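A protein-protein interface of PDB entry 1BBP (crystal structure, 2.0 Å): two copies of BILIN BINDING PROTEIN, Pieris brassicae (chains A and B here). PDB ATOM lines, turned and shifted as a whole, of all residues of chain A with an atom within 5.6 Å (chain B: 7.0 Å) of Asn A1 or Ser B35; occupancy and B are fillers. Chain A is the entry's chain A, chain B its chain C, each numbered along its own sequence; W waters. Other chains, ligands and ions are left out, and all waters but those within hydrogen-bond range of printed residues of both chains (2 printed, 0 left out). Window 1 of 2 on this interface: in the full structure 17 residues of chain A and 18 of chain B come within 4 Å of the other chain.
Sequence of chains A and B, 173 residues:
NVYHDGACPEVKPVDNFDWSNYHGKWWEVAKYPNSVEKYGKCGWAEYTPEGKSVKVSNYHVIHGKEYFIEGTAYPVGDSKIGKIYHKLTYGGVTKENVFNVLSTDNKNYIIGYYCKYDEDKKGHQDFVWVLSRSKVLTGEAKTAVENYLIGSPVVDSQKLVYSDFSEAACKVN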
ATOM      1  N   ASN A   1      -8.869  -1.521 -16.771  1.00  0.00           N
ATOM      2  CA  ASN A   1      -9.762  -1.113 -15.688  1.00  0.00           C
ATOM      3  C   ASN A   1      -9.060   0.033 -14.987  1.00  0.00           C
ATOM      4  O   ASN A   1      -7.826   0.006 -14.925  1.00  0.00           O
ATOM      5  CB  ASN A   1      -9.985  -2.193 -14.633  1.00  0.00           C
ATOM      6  CG  ASN A   1     -10.649  -3.435 -15.213  1.00  0.00           C
ATOM      7  OD1 ASN A   1     -11.100  -4.280 -14.448  1.00  0.00           O
ATOM      8  ND2 ASN A   1     -10.702  -3.553 -16.516  1.00  0.00           N
ATOM      9  N   VAL A   2      -9.831   1.056 -14.657  1.00  0.00           N
ATOM     10  CA  VAL A   2      -9.299   2.327 -14.135  1.00  0.00           C
ATOM     11  C   VAL A   2      -9.739   2.530 -12.689  1.00  0.00           C
ATOM     12  O   VAL A   2     -10.931   2.741 -12.446  1.00  0.00           O
ATOM     13  CB  VAL A   2      -9.788   3.483 -15.037  1.00  0.00           C
ATOM     14  CG1 VAL A   2      -9.344   4.883 -14.549  1.00  0.00           C
ATOM     15  CG2 VAL A   2      -9.447   3.243 -16.538  1.00  0.00           C
ATOM     16  N   TYR A   3      -8.788   2.317 -11.765  1.00  0.00           N
ATOM     17  CA  TYR A   3      -9.033   2.346 -10.306  1.00  0.00           C
ATOM     18  C   TYR A   3      -8.526   3.641  -9.683  1.00  0.00           C
ATOM     19  O   TYR A   3      -7.451   4.093 -10.046  1.00  0.00           O
ATOM     20  CB  TYR A   3      -8.278   1.198  -9.614  1.00  0.00           C
ATOM     21  CG  TYR A   3      -8.625  -0.175 -10.220  1.00  0.00           C
ATOM     22  CD1 TYR A   3      -9.899  -0.679 -10.050  1.00  0.00           C
ATOM     23  CD2 TYR A   3      -7.658  -0.922 -10.867  1.00  0.00           C
ATOM     24  CE1 TYR A   3     -10.227  -1.925 -10.538  1.00  0.00           C
ATOM     25  CE2 TYR A   3      -7.976  -2.178 -11.368  1.00  0.00           C
ATOM     26  CZ  TYR A   3      -9.272  -2.673 -11.207  1.00  0.00           C
ATOM     27  OH  TYR A   3      -9.644  -3.852 -11.808  1.00  0.00           O
ATOM     28  N   PRO A  33     -11.653   0.785 -20.475  1.00  0.00           N
ATOM     29  CA  PRO A  33     -11.702  -0.682 -20.387  1.00  0.00           C
ATOM     30  C   PRO A  33     -12.233  -1.199 -19.048  1.00  0.00           C
ATOM     31  O   PRO A  33     -12.126  -0.544 -18.009  1.00  0.00           O
ATOM     32  CB  PRO A  33     -10.268  -1.134 -20.639  1.00  0.00           C
ATOM     33  CG  PRO A  33      -9.512   0.101 -21.094  1.00  0.00           C
ATOM     34  CD  PRO A  33     -10.311   1.324 -20.654  1.00  0.00           C
ATOM     35  N   ASN A  34     -12.886  -2.330 -19.122  1.00  0.00           N
ATOM     36  CA  ASN A  34     -13.470  -2.975 -17.941  1.00  0.00           C
ATOM     37  C   ASN A  34     -13.395  -4.480 -18.139  1.00  0.00           C
ATOM     38  O   ASN A  34     -13.263  -4.927 -19.278  1.00  0.00           O
ATOM     39  CB  ASN A  34     -14.920  -2.515 -17.641  1.00  0.00           C
ATOM     40  CG  ASN A  34     -15.949  -2.870 -18.725  1.00  0.00           C
ATOM     41  OD1 ASN A  34     -16.241  -4.038 -18.963  1.00  0.00           O
ATOM     42  ND2 ASN A  34     -16.546  -1.861 -19.323  1.00  0.00           N
ATOM     43  N   SER A  35     -13.493  -5.210 -17.044  1.00  0.00           N
ATOM     44  CA  SER A  35     -13.363  -6.665 -17.110  1.00  0.00           C
ATOM     45  C   SER A  35     -14.530  -7.330 -17.826  1.00  0.00           C
ATOM     46  O   SER A  35     -14.360  -8.449 -18.298  1.00  0.00           O
ATOM     47  CB  SER A  35     -13.272  -7.274 -15.687  1.00  0.00           C
ATOM     48  OG  SER A  35     -12.149  -6.755 -14.969  1.00  0.00           O
ATOM     49  N   GLN A 125     -13.716   2.213  -8.936  1.00  0.00           N
ATOM     50  CA  GLN A 125     -13.444   2.055 -10.371  1.00  0.00           C
ATOM     51  C   GLN A 125     -14.357   2.936 -11.219  1.00  0.00           C
ATOM     52  O   GLN A 125     -15.575   2.981 -11.013  1.00  0.00           O
ATOM     53  CB  GLN A 125     -13.686   0.600 -10.796  1.00  0.00           C
ATOM     54  CG  GLN A 125     -13.229   0.326 -12.229  1.00  0.00           C
ATOM     55  CD  GLN A 125     -13.477  -1.114 -12.669  1.00  0.00           C
ATOM     56  OE1 GLN A 125     -13.220  -1.457 -13.823  1.00  0.00           O
ATOM     57  NE2 GLN A 125     -13.966  -1.991 -11.812  1.00  0.00           N
ATOM     58  N   ASN B   1      -6.204  -2.856 -15.806  1.00  0.00           N
ATOM     59  CA  ASN B   1      -6.024  -4.183 -16.385  1.00  0.00           C
ATOM     60  C   ASN B   1      -5.783  -4.047 -17.878  1.00  0.00           C
ATOM     61  O   ASN B   1      -6.384  -3.194 -18.534  1.00  0.00           O
ATOM     62  CB  ASN B   1      -7.249  -5.080 -16.166  1.00  0.00           C
ATOM     63  CG  ASN B   1      -7.534  -5.338 -14.686  1.00  0.00           C
ATOM     64  OD1 ASN B   1      -8.001  -6.430 -14.361  1.00  0.00           O
ATOM     65  ND2 ASN B   1      -7.322  -4.365 -13.821  1.00  0.00           N
ATOM     66  N   VAL B   2      -4.870  -4.850 -18.362  1.00  0.00           N
ATOM     67  CA  VAL B   2      -4.422  -4.735 -19.758  1.00  0.00           C
ATOM     68  C   VAL B   2      -4.793  -5.964 -20.590  1.00  0.00           C
ATOM     69  O   VAL B   2      -4.355  -7.085 -20.331  1.00  0.00           O
ATOM     70  CB  VAL B   2      -2.905  -4.431 -19.786  1.00  0.00           C
ATOM     71  CG1 VAL B   2      -2.326  -4.489 -21.208  1.00  0.00           C
ATOM     72  CG2 VAL B   2      -2.595  -3.073 -19.094  1.00  0.00           C
ATOM     73  N   TYR B   3      -5.699  -5.748 -21.518  1.00  0.00           N
ATOM     74  CA  TYR B   3      -6.220  -6.857 -22.318  1.00  0.00           C
ATOM     75  C   TYR B   3      -5.750  -6.702 -23.755  1.00  0.00           C
ATOM     76  O   TYR B   3      -5.886  -5.611 -24.292  1.00  0.00           O
ATOM     77  CB  TYR B   3      -7.761  -6.809 -22.328  1.00  0.00           C
ATOM     78  CG  TYR B   3      -8.328  -6.921 -20.899  1.00  0.00           C
ATOM     79  CD1 TYR B   3      -8.188  -8.096 -20.201  1.00  0.00           C
ATOM     80  CD2 TYR B   3      -8.930  -5.835 -20.304  1.00  0.00           C
ATOM     81  CE1 TYR B   3      -8.670  -8.188 -18.907  1.00  0.00           C
ATOM     82  CE2 TYR B   3      -9.428  -5.926 -19.016  1.00  0.00           C
ATOM     83  CZ  TYR B   3      -9.303  -7.103 -18.333  1.00  0.00           C
ATOM     84  OH  TYR B   3      -9.764  -7.191 -17.065  1.00  0.00           O
ATOM     85  N   TYR B  32       1.585  -3.057 -14.155  1.00  0.00           N
ATOM     86  CA  TYR B  32       0.316  -2.914 -14.875  1.00  0.00           C
ATOM     87  C   TYR B  32      -0.762  -3.218 -13.853  1.00  0.00           C
ATOM     88  O   TYR B  32      -0.630  -4.246 -13.199  1.00  0.00           O
ATOM     89  CB  TYR B  32       0.138  -4.018 -15.901  1.00  0.00           C
ATOM     90  CG  TYR B  32       0.835  -3.741 -17.242  1.00  0.00           C
ATOM     91  CD1 TYR B  32       0.561  -4.598 -18.275  1.00  0.00           C
ATOM     92  CD2 TYR B  32       1.737  -2.711 -17.409  1.00  0.00           C
ATOM     93  CE1 TYR B  32       1.166  -4.429 -19.492  1.00  0.00           C
ATOM     94  CE2 TYR B  32       2.365  -2.533 -18.640  1.00  0.00           C
ATOM     95  CZ  TYR B  32       2.062  -3.399 -19.680  1.00  0.00           C
ATOM     96  OH  TYR B  32       2.670  -3.286 -20.900  1.00  0.00           O
ATOM     97  N   PRO B  33      -1.773  -2.362 -13.760  1.00  0.00           N
ATOM     98  CA  PRO B  33      -2.896  -2.624 -12.867  1.00  0.00           C
ATOM     99  C   PRO B  33      -3.590  -3.946 -13.187  1.00  0.00           C
ATOM    100  O   PRO B  33      -3.677  -4.363 -14.343  1.00  0.00           O
ATOM    101  CB  PRO B  33      -3.833  -1.431 -13.080  1.00  0.00           C
ATOM    102  CG  PRO B  33      -3.023  -0.363 -13.774  1.00  0.00           C
ATOM    103  CD  PRO B  33      -1.902  -1.080 -14.493  1.00  0.00           C
ATOM    104  N   ASN B  34      -3.952  -4.629 -12.124  1.00  0.00           N
ATOM    105  CA  ASN B  34      -4.703  -5.879 -12.203  1.00  0.00           C
ATOM    106  C   ASN B  34      -5.768  -5.868 -11.105  1.00  0.00           C
ATOM    107  O   ASN B  34      -5.803  -4.955 -10.276  1.00  0.00           O
ATOM    108  CB  ASN B  34      -3.786  -7.126 -12.141  1.00  0.00           C
ATOM    109  CG  ASN B  34      -2.971  -7.175 -10.836  1.00  0.00           C
ATOM    110  OD1 ASN B  34      -1.751  -6.986 -10.844  1.00  0.00           O
ATOM    111  ND2 ASN B  34      -3.633  -7.430  -9.744  1.00  0.00           N
ATOM    112  N   SER B  35      -6.734  -6.716 -11.225  1.00  0.00           N
ATOM    113  CA  SER B  35      -7.849  -6.650 -10.274  1.00  0.00           C
ATOM    114  C   SER B  35      -7.447  -7.126  -8.870  1.00  0.00           C
ATOM    115  O   SER B  35      -8.045  -6.666  -7.906  1.00  0.00           O
ATOM    116  CB  SER B  35      -9.014  -7.542 -10.769  1.00  0.00           C
ATOM    117  OG  SER B  35      -9.613  -7.036 -11.970  1.00  0.00           O
ATOM    118  N   VAL B  36      -6.552  -8.104  -8.731  1.00  0.00           N
ATOM    119  CA  VAL B  36      -6.207  -8.623  -7.380  1.00  0.00           C
ATOM    120  C   VAL B  36      -5.562  -7.551  -6.494  1.00  0.00           C
ATOM    121  O   VAL B  36      -5.809  -7.431  -5.291  1.00  0.00           O
ATOM    122  CB  VAL B  36      -5.249  -9.805  -7.553  1.00  0.00           C
ATOM    123  CG1 VAL B  36      -4.321  -9.986  -6.361  1.00  0.00           C
ATOM    124  CG2 VAL B  36      -5.977 -11.119  -7.886  1.00  0.00           C
ATOM    125  N   GLU B  37      -4.854  -6.660  -7.117  1.00  0.00           N
ATOM    126  CA  GLU B  37      -4.123  -5.687  -6.325  1.00  0.00           C
ATOM    127  C   GLU B  37      -4.755  -4.313  -6.349  1.00  0.00           C
ATOM    128  O   GLU B  37      -4.087  -3.358  -5.966  1.00  0.00           O
ATOM    129  CB  GLU B  37      -2.732  -5.550  -6.917  1.00  0.00           C
ATOM    130  CG  GLU B  37      -1.915  -6.849  -6.808  1.00  0.00           C
ATOM    131  CD  GLU B  37      -0.501  -6.477  -7.255  1.00  0.00           C
ATOM    132  OE1 GLU B  37       0.018  -7.042  -8.246  1.00  0.00           O
ATOM    133  OE2 GLU B  37       0.089  -5.580  -6.611  1.00  0.00           O
ATOM    134  N   LYS B  38      -5.991  -4.238  -6.786  1.00  0.00           N
ATOM    135  CA  LYS B  38      -6.632  -2.921  -6.845  1.00  0.00           C
ATOM    136  C   LYS B  38      -6.678  -2.255  -5.478  1.00  0.00           C
ATOM    137  O   LYS B  38      -6.954  -2.923  -4.480  1.00  0.00           O
ATOM    138  CB  LYS B  38      -8.035  -2.946  -7.505  1.00  0.00           C
ATOM    139  CG  LYS B  38      -9.059  -3.810  -6.763  1.00  0.00           C
ATOM    140  CD  LYS B  38     -10.374  -3.896  -7.533  1.00  0.00           C
ATOM    141  CE  LYS B  38     -11.275  -4.993  -6.939  1.00  0.00           C
ATOM    142  NZ  LYS B  38     -12.520  -5.129  -7.723  1.00  0.00           N
ATOM    143  N   TYR B  39      -6.394  -0.969  -5.521  1.00  0.00           N
ATOM    144  CA  TYR B  39      -6.437  -0.056  -4.372  1.00  0.00           C
ATOM    145  C   TYR B  39      -5.275  -0.264  -3.393  1.00  0.00           C
ATOM    146  O   TYR B  39      -5.136   0.516  -2.444  1.00  0.00           O
ATOM    147  CB  TYR B  39      -7.776  -0.133  -3.596  1.00  0.00           C
ATOM    148  CG  TYR B  39      -9.019  -0.063  -4.501  1.00  0.00           C
ATOM    149  CD1 TYR B  39      -9.023   0.766  -5.601  1.00  0.00           C
ATOM    150  CD2 TYR B  39     -10.096  -0.887  -4.253  1.00  0.00           C
ATOM    151  CE1 TYR B  39     -10.101   0.759  -6.470  1.00  0.00           C
ATOM    152  CE2 TYR B  39     -11.172  -0.900  -5.118  1.00  0.00           C
ATOM    153  CZ  TYR B  39     -11.160  -0.075  -6.238  1.00  0.00           C
ATOM    154  OH  TYR B  39     -12.208  -0.060  -7.099  1.00  0.00           O
ATOM    155  N   GLN B 125      -4.584 -11.396 -20.941  1.00  0.00           N
ATOM    156  CA  GLN B 125      -4.353 -10.270 -20.033  1.00  0.00           C
ATOM    157  C   GLN B 125      -2.874 -10.200 -19.695  1.00  0.00           C
ATOM    158  O   GLN B 125      -2.228 -11.216 -19.421  1.00  0.00           O
ATOM    159  CB  GLN B 125      -5.140 -10.360 -18.696  1.00  0.00           C
ATOM    160  CG  GLN B 125      -4.990  -9.083 -17.856  1.00  0.00           C
ATOM    161  CD  GLN B 125      -5.672  -9.158 -16.488  1.00  0.00           C
ATOM    162  OE1 GLN B 125      -5.567  -8.220 -15.695  1.00  0.00           O
ATOM    163  NE2 GLN B 125      -6.372 -10.225 -16.158  1.00  0.00           N
ATOM    164  N   PHE B 127       0.242  -8.960 -17.400  1.00  0.00           N
ATOM    165  CA  PHE B 127       0.692  -8.588 -16.075  1.00  0.00           C
ATOM    166  C   PHE B 127       2.176  -8.236 -16.139  1.00  0.00           C
ATOM    167  O   PHE B 127       2.972  -9.031 -16.633  1.00  0.00           O
ATOM    168  CB  PHE B 127       0.577  -9.654 -15.140  1.00  0.00           C
ATOM    169  CG  PHE B 127      -0.803 -10.104 -14.919  1.00  0.00           C
ATOM    170  CD1 PHE B 127      -1.497 -10.765 -15.918  1.00  0.00           C
ATOM    171  CD2 PHE B 127      -1.326  -9.825 -13.675  1.00  0.00           C
ATOM    172  CE1 PHE B 127      -2.771 -11.238 -15.628  1.00  0.00           C
ATOM    173  CE2 PHE B 127      -2.588 -10.318 -13.370  1.00  0.00           C
ATOM    174  CZ  PHE B 127      -3.311 -11.032 -14.345  1.00  0.00           C
HETATM  175  O   HOH W   1     -12.888  -8.018 -12.267  1.00  0.00           O
HETATM  176  O   HOH W   2     -14.025  -2.752  -8.844  1.00  0.00           O
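Asn A1 touches Tyr B3, and with the chains exchanged Tyr A3 touches Asn B1.
Asn A1 touches Ser B35, but with the chains exchanged Ser A35 does not touch Asn B1 (4.2 Å).
Tyr A3 touches Ser B35, and with the chains exchanged Ser A35 touches Tyr B3.
Ser B35 touches its own counterpart, Ser A35.
The side-chain amide oxygen (OD1) of Asn A1 lies within hydrogen-bond range of the side-chain hydroxyl (OH) of Tyr A3, 3.0 Å away.
OD1 of Asn B1 is in hydrogen-bond range of OH of Tyr B3.
The side-chain hydroxyl (OG) of Ser B35 lies within hydrogen-bond range of the side-chain amide oxygen (OD1) of Asn B1 (2.9 Å).
OE1 of Gln B125 lies close to OD1 of Asn B1 (3.3 Å).
N of Val B36 lies close to ND2 of Asn B34, at 3.2 Å.
The side-chain amide nitrogen of Asn B34 lies close to the backbone NH of Glu B37.
Printed residues of chain B within 4 Å of Asn A34: Tyr B3 (3.97 Å).
Of the printed residues of chain A, Asn B1 touches Asn A1 and Tyr A3.
The nearest printed residue of chain B that does not touch Asn A1 is Pro B33 (4.6 Å).
The nearest printed residue of chain A that does not touch Ser B35 is Gln A125 (6.7 Å).
The nearest printed residue of chain A that does not touch Tyr B3 is Pro A33 (4.9 Å).
Water W2 bridges NZ of Lys B38 and NE2 of Gln A125.
Water W1 bridges OG of Ser A35 and OG of Ser B35.
The backbone carbonyl oxygen (O) of Asn A1 sits at hydrogen-bond distance from the backbone NH (N) of Asn B1.
The side-chain amide nitrogen (ND2) of Asn B1 sits at hydrogen-bond distance from the side-chain hydroxyl (OH) of Tyr A3 (3.1 Å).
OH of Tyr A3 sits at hydrogen-bond distance from OG of Ser B35.
OG of Ser A35 is in hydrogen-bond range of OH of Tyr B3, at 3.2 Å.
N of Gln A125 is in hydrogen-bond range of OH of Tyr B39, at 3.3 Å.
Among the printed residues, pairs that only touch across the chains: Asn A1 with Tyr B3, Asn A1 with Ser B35, Tyr A3 with Asn B34, Tyr A3 with Lys B38, Tyr A3 with Tyr B39, Asn A34 with Tyr B3 and Ser A35 with Ser B35.
Printed residues of chain A that touch a printed residue of chain B: Asn A1, Tyr A3, Asn A34, Ser A35 and Gln A125.
Hydrophobic or aromatic side chains of chain A within 4 Å of the printed part of chain B: Tyr A3.
Among the printed residues, 12 pairs touch across the chains.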
